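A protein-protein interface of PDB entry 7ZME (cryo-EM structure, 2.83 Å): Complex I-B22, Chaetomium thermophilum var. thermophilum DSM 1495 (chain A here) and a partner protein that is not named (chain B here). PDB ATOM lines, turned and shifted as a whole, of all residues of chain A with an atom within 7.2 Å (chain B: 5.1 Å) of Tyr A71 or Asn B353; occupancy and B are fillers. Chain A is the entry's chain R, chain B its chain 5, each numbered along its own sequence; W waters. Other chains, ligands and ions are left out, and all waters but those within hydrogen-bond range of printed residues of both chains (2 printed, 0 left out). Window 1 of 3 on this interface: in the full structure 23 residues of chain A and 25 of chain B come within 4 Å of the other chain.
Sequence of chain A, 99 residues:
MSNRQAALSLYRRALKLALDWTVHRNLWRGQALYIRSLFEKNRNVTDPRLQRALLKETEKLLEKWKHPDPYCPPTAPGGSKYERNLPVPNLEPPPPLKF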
ATOM      1  N   LYS A  16     -24.888 -23.305   1.076  1.00  0.00           N
ATOM      2  CA  LYS A  16     -25.195 -22.245   2.067  1.00  0.00           C
ATOM      3  C   LYS A  16     -26.221 -22.755   3.066  1.00  0.00           C
ATOM      4  O   LYS A  16     -26.058 -22.468   4.248  1.00  0.00           O
ATOM      5  CB  LYS A  16     -25.657 -20.974   1.357  1.00  0.00           C
ATOM      6  CG  LYS A  16     -24.539 -20.084   0.836  1.00  0.00           C
ATOM      7  CD  LYS A  16     -25.026 -18.737   0.353  1.00  0.00           C
ATOM      8  CE  LYS A  16     -25.655 -17.910   1.454  1.00  0.00           C
ATOM      9  NZ  LYS A  16     -26.116 -16.592   0.960  1.00  0.00           N
ATOM     10  N   LEU A  19     -24.701 -25.483   5.649  1.00  0.00           N
ATOM     11  CA  LEU A  19     -23.991 -24.775   6.743  1.00  0.00           C
ATOM     12  C   LEU A  19     -25.003 -24.029   7.616  1.00  0.00           C
ATOM     13  O   LEU A  19     -24.826 -24.023   8.832  1.00  0.00           O
ATOM     14  CB  LEU A  19     -22.960 -23.819   6.128  1.00  0.00           C
ATOM     15  CG  LEU A  19     -21.870 -23.310   7.071  1.00  0.00           C
ATOM     16  CD1 LEU A  19     -21.285 -24.432   7.911  1.00  0.00           C
ATOM     17  CD2 LEU A  19     -20.774 -22.594   6.302  1.00  0.00           C
ATOM     18  N   ASP A  20     -26.025 -23.408   7.036  1.00  0.00           N
ATOM     19  CA  ASP A  20     -26.963 -22.586   7.852  1.00  0.00           C
ATOM     20  C   ASP A  20     -27.630 -23.488   8.878  1.00  0.00           C
ATOM     21  O   ASP A  20     -27.827 -23.015   9.995  1.00  0.00           O
ATOM     22  CB  ASP A  20     -27.994 -21.825   7.021  1.00  0.00           C
ATOM     23  CG  ASP A  20     -27.440 -20.628   6.279  1.00  0.00           C
ATOM     24  OD1 ASP A  20     -26.406 -20.093   6.722  1.00  0.00           O
ATOM     25  OD2 ASP A  20     -28.045 -20.251   5.255  1.00  0.00           O
ATOM     26  N   HIS A  67     -33.965 -22.665   5.973  1.00  0.00           N
ATOM     27  CA  HIS A  67     -33.702 -22.322   7.358  1.00  0.00           C
ATOM     28  C   HIS A  67     -34.654 -21.220   7.816  1.00  0.00           C
ATOM     29  O   HIS A  67     -35.009 -20.337   7.028  1.00  0.00           O
ATOM     30  CB  HIS A  67     -32.253 -21.869   7.532  1.00  0.00           C
ATOM     31  CG  HIS A  67     -31.725 -22.074   8.915  1.00  0.00           C
ATOM     32  ND1 HIS A  67     -31.701 -21.072   9.857  1.00  0.00           N
ATOM     33  CD2 HIS A  67     -31.226 -23.175   9.523  1.00  0.00           C
ATOM     34  CE1 HIS A  67     -31.200 -21.543  10.985  1.00  0.00           C
ATOM     35  NE2 HIS A  67     -30.902 -22.816  10.808  1.00  0.00           N
ATOM     36  N   ASP A  69     -33.979 -18.728   9.671  1.00  0.00           N
ATOM     37  CA  ASP A  69     -33.221 -17.501   9.442  1.00  0.00           C
ATOM     38  C   ASP A  69     -31.824 -17.865   8.952  1.00  0.00           C
ATOM     39  O   ASP A  69     -31.020 -18.444   9.699  1.00  0.00           O
ATOM     40  CB  ASP A  69     -33.183 -16.621  10.689  1.00  0.00           C
ATOM     41  CG  ASP A  69     -32.428 -17.250  11.840  1.00  0.00           C
ATOM     42  OD1 ASP A  69     -32.500 -18.487  12.002  1.00  0.00           O
ATOM     43  OD2 ASP A  69     -31.762 -16.502  12.586  1.00  0.00           O
ATOM     44  N   PRO A  70     -31.478 -17.613   7.659  1.00  0.00           N
ATOM     45  CA  PRO A  70     -30.119 -17.857   7.170  1.00  0.00           C
ATOM     46  C   PRO A  70     -29.052 -16.868   7.650  1.00  0.00           C
ATOM     47  O   PRO A  70     -29.402 -15.775   8.017  1.00  0.00           O
ATOM     48  CB  PRO A  70     -30.245 -17.656   5.660  1.00  0.00           C
ATOM     49  CG  PRO A  70     -31.699 -17.864   5.377  1.00  0.00           C
ATOM     50  CD  PRO A  70     -32.342 -17.168   6.549  1.00  0.00           C
ATOM     51  N   TYR A  71     -27.785 -17.266   7.627  1.00  0.00           N
ATOM     52  CA  TYR A  71     -26.694 -16.330   8.007  1.00  0.00           C
ATOM     53  C   TYR A  71     -26.576 -15.184   6.992  1.00  0.00           C
ATOM     54  O   TYR A  71     -26.719 -15.427   5.783  1.00  0.00           O
ATOM     55  CB  TYR A  71     -25.360 -17.040   8.252  1.00  0.00           C
ATOM     56  CG  TYR A  71     -24.162 -16.131   8.191  1.00  0.00           C
ATOM     57  CD1 TYR A  71     -23.705 -15.473   9.319  1.00  0.00           C
ATOM     58  CD2 TYR A  71     -23.501 -15.906   6.997  1.00  0.00           C
ATOM     59  CE1 TYR A  71     -22.616 -14.621   9.267  1.00  0.00           C
ATOM     60  CE2 TYR A  71     -22.408 -15.060   6.927  1.00  0.00           C
ATOM     61  CZ  TYR A  71     -21.964 -14.414   8.066  1.00  0.00           C
ATOM     62  OH  TYR A  71     -20.887 -13.580   8.008  1.00  0.00           O
ATOM     63  N   CYS A  72     -26.305 -13.979   7.481  1.00  0.00           N
ATOM     64  CA  CYS A  72     -26.170 -12.790   6.616  1.00  0.00           C
ATOM     65  C   CYS A  72     -25.074 -11.902   7.225  1.00  0.00           C
ATOM     66  O   CYS A  72     -25.281 -11.414   8.344  1.00  0.00           O
ATOM     67  CB  CYS A  72     -27.469 -11.999   6.560  1.00  0.00           C
ATOM     68  SG  CYS A  72     -27.586 -10.875   5.147  1.00  0.00           S
ATOM     69  N   PRO A  73     -23.904 -11.693   6.580  1.00  0.00           N
ATOM     70  CA  PRO A  73     -22.837 -10.868   7.159  1.00  0.00           C
ATOM     71  C   PRO A  73     -23.362  -9.503   7.566  1.00  0.00           C
ATOM     72  O   PRO A  73     -24.296  -8.979   6.944  1.00  0.00           O
ATOM     73  CB  PRO A  73     -21.808 -10.762   6.021  1.00  0.00           C
ATOM     74  CG  PRO A  73     -22.493 -11.272   4.807  1.00  0.00           C
ATOM     75  CD  PRO A  73     -23.549 -12.211   5.252  1.00  0.00           C
ATOM     76  N   PRO A  74     -22.796  -8.902   8.614  1.00  0.00           N
ATOM     77  CA  PRO A  74     -23.407  -7.687   9.182  1.00  0.00           C
ATOM     78  C   PRO A  74     -23.540  -6.543   8.196  1.00  0.00           C
ATOM     79  O   PRO A  74     -24.491  -5.761   8.295  1.00  0.00           O
ATOM     80  CB  PRO A  74     -22.460  -7.328  10.333  1.00  0.00           C
ATOM     81  CG  PRO A  74     -21.743  -8.602  10.653  1.00  0.00           C
ATOM     82  CD  PRO A  74     -21.594  -9.319   9.355  1.00  0.00           C
ATOM     83  N   ALA A  76     -23.967  -6.964   4.930  1.00  0.00           N
ATOM     84  CA  ALA A  76     -24.818  -7.395   3.836  1.00  0.00           C
ATOM     85  C   ALA A  76     -26.248  -6.915   4.041  1.00  0.00           C
ATOM     86  O   ALA A  76     -26.663  -6.640   5.167  1.00  0.00           O
ATOM     87  CB  ALA A  76     -24.791  -8.913   3.723  1.00  0.00           C
ATOM     88  N   SER A  80     -26.730  -7.181  10.486  1.00  0.00           N
ATOM     89  CA  SER A  80     -26.990  -6.358  11.663  1.00  0.00           C
ATOM     90  C   SER A  80     -26.472  -4.934  11.508  1.00  0.00           C
ATOM     91  O   SER A  80     -27.087  -3.996  12.020  1.00  0.00           O
ATOM     92  CB  SER A  80     -26.369  -7.011  12.893  1.00  0.00           C
ATOM     93  OG  SER A  80     -26.829  -8.338  13.047  1.00  0.00           O
ATOM     94  N   LYS A  81     -25.347  -4.752  10.825  1.00  0.00           N
ATOM     95  CA  LYS A  81     -24.690  -3.459  10.706  1.00  0.00           C
ATOM     96  C   LYS A  81     -25.076  -2.722   9.426  1.00  0.00           C
ATOM     97  O   LYS A  81     -24.536  -1.649   9.150  1.00  0.00           O
ATOM     98  CB  LYS A  81     -23.170  -3.660  10.775  1.00  0.00           C
ATOM     99  CG  LYS A  81     -22.339  -2.406  10.940  1.00  0.00           C
ATOM    100  CD  LYS A  81     -20.888  -2.673  10.617  1.00  0.00           C
ATOM    101  CE  LYS A  81     -20.013  -2.530  11.837  1.00  0.00           C
ATOM    102  NZ  LYS A  81     -18.584  -2.343  11.470  1.00  0.00           N
ATOM    103  N   ILE B 347     -19.045  -8.868  20.335  1.00  0.00           N
ATOM    104  CA  ILE B 347     -19.409  -8.292  19.042  1.00  0.00           C
ATOM    105  C   ILE B 347     -18.365  -7.281  18.589  1.00  0.00           C
ATOM    106  O   ILE B 347     -18.050  -7.193  17.398  1.00  0.00           O
ATOM    107  CB  ILE B 347     -20.827  -7.684  19.084  1.00  0.00           C
ATOM    108  CG1 ILE B 347     -21.891  -8.753  19.343  1.00  0.00           C
ATOM    109  CG2 ILE B 347     -21.144  -6.931  17.810  1.00  0.00           C
ATOM    110  CD1 ILE B 347     -22.208  -9.031  20.763  1.00  0.00           C
ATOM    111  N   VAL B 350     -14.970  -9.175  17.250  1.00  0.00           N
ATOM    112  CA  VAL B 350     -15.166  -9.590  15.868  1.00  0.00           C
ATOM    113  C   VAL B 350     -15.672  -8.392  15.078  1.00  0.00           C
ATOM    114  O   VAL B 350     -15.976  -7.343  15.653  1.00  0.00           O
ATOM    115  CB  VAL B 350     -16.129 -10.783  15.774  1.00  0.00           C
ATOM    116  CG1 VAL B 350     -15.607 -11.935  16.610  1.00  0.00           C
ATOM    117  CG2 VAL B 350     -17.518 -10.383  16.224  1.00  0.00           C
ATOM    118  N   ALA B 351     -15.737  -8.517  13.757  1.00  0.00           N
ATOM    119  CA  ALA B 351     -16.202  -7.400  12.946  1.00  0.00           C
ATOM    120  C   ALA B 351     -17.700  -7.197  13.122  1.00  0.00           C
ATOM    121  O   ALA B 351     -18.470  -7.325  12.166  1.00  0.00           O
ATOM    122  CB  ALA B 351     -15.864  -7.628  11.471  1.00  0.00           C
ATOM    123  N   ASP B 352     -18.112  -6.877  14.351  1.00  0.00           N
ATOM    124  CA  ASP B 352     -19.504  -6.587  14.693  1.00  0.00           C
ATOM    125  C   ASP B 352     -20.453  -7.704  14.265  1.00  0.00           C
ATOM    126  O   ASP B 352     -21.627  -7.470  13.979  1.00  0.00           O
ATOM    127  CB  ASP B 352     -19.951  -5.243  14.118  1.00  0.00           C
ATOM    128  CG  ASP B 352     -19.533  -4.077  14.992  1.00  0.00           C
ATOM    129  OD1 ASP B 352     -18.647  -4.272  15.851  1.00  0.00           O
ATOM    130  OD2 ASP B 352     -20.108  -2.978  14.847  1.00  0.00           O
ATOM    131  N   ASN B 353     -19.947  -8.930  14.227  1.00  0.00           N
ATOM    132  CA  ASN B 353     -20.790 -10.086  13.979  1.00  0.00           C
ATOM    133  C   ASN B 353     -21.622 -10.403  15.214  1.00  0.00           C
ATOM    134  O   ASN B 353     -21.161 -10.263  16.347  1.00  0.00           O
ATOM    135  CB  ASN B 353     -19.937 -11.292  13.595  1.00  0.00           C
ATOM    136  CG  ASN B 353     -20.769 -12.479  13.183  1.00  0.00           C
ATOM    137  OD1 ASN B 353     -21.515 -12.421  12.207  1.00  0.00           O
ATOM    138  ND2 ASN B 353     -20.649 -13.570  13.928  1.00  0.00           N
ATOM    139  N   GLN B 354     -22.859 -10.836  14.987  1.00  0.00           N
ATOM    140  CA  GLN B 354     -23.752 -11.195  16.076  1.00  0.00           C
ATOM    141  C   GLN B 354     -24.333 -12.590  15.908  1.00  0.00           C
ATOM    142  O   GLN B 354     -25.279 -12.942  16.618  1.00  0.00           O
ATOM    143  CB  GLN B 354     -24.884 -10.170  16.200  1.00  0.00           C
ATOM    144  CG  GLN B 354     -24.504  -8.914  16.941  1.00  0.00           C
ATOM    145  CD  GLN B 354     -25.163  -7.686  16.367  1.00  0.00           C
ATOM    146  OE1 GLN B 354     -24.535  -6.638  16.235  1.00  0.00           O
ATOM    147  NE2 GLN B 354     -26.438  -7.804  16.021  1.00  0.00           N
ATOM    148  N   ASP B 355     -23.796 -13.387  14.994  1.00  0.00           N
ATOM    149  CA  ASP B 355     -24.281 -14.735  14.739  1.00  0.00           C
ATOM    150  C   ASP B 355     -23.359 -15.744  15.407  1.00  0.00           C
ATOM    151  O   ASP B 355     -22.136 -15.665  15.261  1.00  0.00           O
ATOM    152  CB  ASP B 355     -24.362 -15.007  13.236  1.00  0.00           C
ATOM    153  CG  ASP B 355     -25.325 -16.124  12.897  1.00  0.00           C
ATOM    154  OD1 ASP B 355     -25.332 -17.146  13.613  1.00  0.00           O
ATOM    155  OD2 ASP B 355     -26.076 -15.982  11.913  1.00  0.00           O
ATOM    156  N   PHE B 356     -23.952 -16.690  16.139  1.00  0.00           N
ATOM    157  CA  PHE B 356     -23.165 -17.739  16.778  1.00  0.00           C
ATOM    158  C   PHE B 356     -22.425 -18.581  15.752  1.00  0.00           C
ATOM    159  O   PHE B 356     -21.361 -19.133  16.052  1.00  0.00           O
ATOM    160  CB  PHE B 356     -24.069 -18.632  17.625  1.00  0.00           C
ATOM    161  CG  PHE B 356     -24.579 -17.977  18.870  1.00  0.00           C
ATOM    162  CD1 PHE B 356     -23.700 -17.453  19.803  1.00  0.00           C
ATOM    163  CD2 PHE B 356     -25.937 -17.889  19.112  1.00  0.00           C
ATOM    164  CE1 PHE B 356     -24.169 -16.854  20.950  1.00  0.00           C
ATOM    165  CE2 PHE B 356     -26.409 -17.291  20.258  1.00  0.00           C
ATOM    166  CZ  PHE B 356     -25.526 -16.776  21.177  1.00  0.00           C
ATOM    167  N   ARG B 357     -22.980 -18.654  14.541  1.00  0.00           N
ATOM    168  CA  ARG B 357     -22.418 -19.533  13.485  1.00  0.00           C
ATOM    169  C   ARG B 357     -21.025 -19.056  13.055  1.00  0.00           C
ATOM    170  O   ARG B 357     -20.427 -19.715  12.200  1.00  0.00           O
ATOM    171  CB  ARG B 357     -23.431 -19.652  12.345  1.00  0.00           C
ATOM    172  CG  ARG B 357     -24.714 -20.372  12.740  1.00  0.00           C
ATOM    173  CD  ARG B 357     -25.866 -20.377  11.748  1.00  0.00           C
ATOM    174  NE  ARG B 357     -26.644 -19.147  11.732  1.00  0.00           N
ATOM    175  CZ  ARG B 357     -27.777 -18.970  11.061  1.00  0.00           C
ATOM    176  NH1 ARG B 357     -28.399 -17.807  11.113  1.00  0.00           N
ATOM    177  NH2 ARG B 357     -28.293 -19.952  10.350  1.00  0.00           N
ATOM    178  N   LYS B 358     -20.531 -17.949  13.602  1.00  0.00           N
ATOM    179  CA  LYS B 358     -19.246 -17.387  13.134  1.00  0.00           C
ATOM    180  C   LYS B 358     -18.294 -17.180  14.300  1.00  0.00           C
ATOM    181  O   LYS B 358     -17.355 -16.404  14.145  1.00  0.00           O
ATOM    182  CB  LYS B 358     -19.518 -16.088  12.388  1.00  0.00           C
ATOM    183  CG  LYS B 358     -20.154 -16.245  11.016  1.00  0.00           C
ATOM    184  CD  LYS B 358     -19.322 -17.084  10.074  1.00  0.00           C
ATOM    185  CE  LYS B 358     -20.174 -17.753   9.023  1.00  0.00           C
ATOM    186  NZ  LYS B 358     -21.353 -18.397   9.645  1.00  0.00           N
ATOM    187  N   PHE B 359     -18.563 -17.821  15.430  1.00  0.00           N
ATOM    188  CA  PHE B 359     -17.711 -17.675  16.632  1.00  0.00           C
ATOM    189  C   PHE B 359     -17.106 -19.025  16.999  1.00  0.00           C
ATOM    190  O   PHE B 359     -17.342 -19.979  16.261  1.00  0.00           O
ATOM    191  CB  PHE B 359     -18.548 -17.181  17.816  1.00  0.00           C
ATOM    192  CG  PHE B 359     -19.252 -15.858  17.665  1.00  0.00           C
ATOM    193  CD1 PHE B 359     -18.641 -14.788  17.036  1.00  0.00           C
ATOM    194  CD2 PHE B 359     -20.514 -15.674  18.200  1.00  0.00           C
ATOM    195  CE1 PHE B 359     -19.298 -13.576  16.917  1.00  0.00           C
ATOM    196  CE2 PHE B 359     -21.167 -14.458  18.089  1.00  0.00           C
ATOM    197  CZ  PHE B 359     -20.557 -13.412  17.442  1.00  0.00           C
ATOM    198  N   TYR B 443     -10.640 -13.268  12.541  1.00  0.00           N
ATOM    199  CA  TYR B 443     -10.929 -13.274  13.967  1.00  0.00           C
ATOM    200  C   TYR B 443      -9.835 -13.933  14.793  1.00  0.00           C
ATOM    201  O   TYR B 443      -9.714 -13.628  15.984  1.00  0.00           O
ATOM    202  CB  TYR B 443     -12.256 -13.988  14.230  1.00  0.00           C
ATOM    203  CG  TYR B 443     -13.468 -13.336  13.607  1.00  0.00           C
ATOM    204  CD1 TYR B 443     -13.416 -12.040  13.124  1.00  0.00           C
ATOM    205  CD2 TYR B 443     -14.669 -14.020  13.512  1.00  0.00           C
ATOM    206  CE1 TYR B 443     -14.523 -11.444  12.561  1.00  0.00           C
ATOM    207  CE2 TYR B 443     -15.782 -13.432  12.951  1.00  0.00           C
ATOM    208  CZ  TYR B 443     -15.703 -12.144  12.477  1.00  0.00           C
ATOM    209  OH  TYR B 443     -16.809 -11.551  11.913  1.00  0.00           O
HETATM  210  O   HOH W   1     -26.806 -13.967  10.443  1.00  0.00           O
HETATM  211  O   HOH W   2     -24.413 -10.200  12.198  1.00  0.00           O
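Water W1 lies within hydrogen-bond range of OD2 of Asp B355 and N of Cys A72.
Water W2 lies within hydrogen-bond range of OG of Ser A80 (3.2 Å) and N of Gln B354 (3.3 Å).
NH2 of Arg B357 is in hydrogen-bond range of O of Asp A20 (3.1 Å).
OD2 of Asp A69 is in salt-bridge range of NH1 of Arg B357 (3.9 Å).
The side-chain amide nitrogen (NE2) of Gln B354 is in hydrogen-bond range of the side-chain hydroxyl (OG) of Ser A80 (3.0 Å).
The side-chain carboxylate of Asp B352 lies within salt-bridge range of the side-chain amino group of Lys A81 (3.8 Å).
Of chain B, only Asn B353 (3.8 Å), Asp B355 (3.6 Å), Arg B357 (3.6 Å) and Lys B358 (3.4 Å) come within 4 Å of Tyr A71.
Asn B353 touches just these residues of chain A: Tyr A71 and Pro A74.
Printed residues of chain A within 4 Å of Asp B355: Tyr A71 (3.6 Å).
Printed residues of chain A within 4 Å of Ala B351: Pro A74.
Printed residues of chain B within 4 Å of Lys A81: Asp B352 (3.0 Å).
Of the printed residues of chain A, Asp B352 touches Pro A74 and Lys A81.
Leu A19 touches none of the printed residues of chain B.
The nearest printed residue of chain B that does not touch Tyr A71 is Tyr B443 (6.0 Å).
The nearest residue of chain A that does not touch Asn B353 is Pro A73 (5.4 Å).
The nearest printed residue of chain A that does not touch Asp B352 is Ser A80 (4.9 Å).
N of Tyr A71 is in hydrogen-bond range of OD1 of Asp A20 (3.3 Å).
The backbone NH (N) of Ser A80 sits at hydrogen-bond distance from the backbone carbonyl oxygen (O) of Pro A74 (3.4 Å).
O of Pro A74 lies within hydrogen-bond range of N of Lys A81 (2.9 Å).
The backbone carbonyl oxygen (O) of Ile B347 sits at hydrogen-bond distance from the backbone NH (N) of Asp B352 (3.1 Å).
The side-chain amide nitrogen (ND2) of Asn B353 is in hydrogen-bond range of the backbone carbonyl oxygen (O) of Asp B355 (2.9 Å).
OD1 of Asp B355 lies within salt-bridge range of NE of Arg B357.
Printed residues of chain B that touch a printed residue of chain A: Ala B351, Asp B352, Asn B353, Gln B354, Asp B355, Arg B357 and Lys B358.
Hydrophobic or aromatic side chains of chain A that line the printed part of chain B: His A67, Tyr A71 and Pro A74.
Among the printed residues, 13 pairs touch across the chains.
Arg B357 touches His A67.
Pro A70 touches Arg B357.
Tyr A71 touches Asn B353.
Tyr A71 touches Asp B355 (CD1 to OD2, 3.6 Å).
Arg B357 touches Tyr A71.
Tyr A71 touches Lys B358 (CE1 to CG, 3.4 Å).
Pro A74 touches Ala B351.
CG of Pro A74 touches O of Asp B352, 3.5 Å away.
Asn B353 touches Pro A74 (CA to CG, 3.8 Å).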
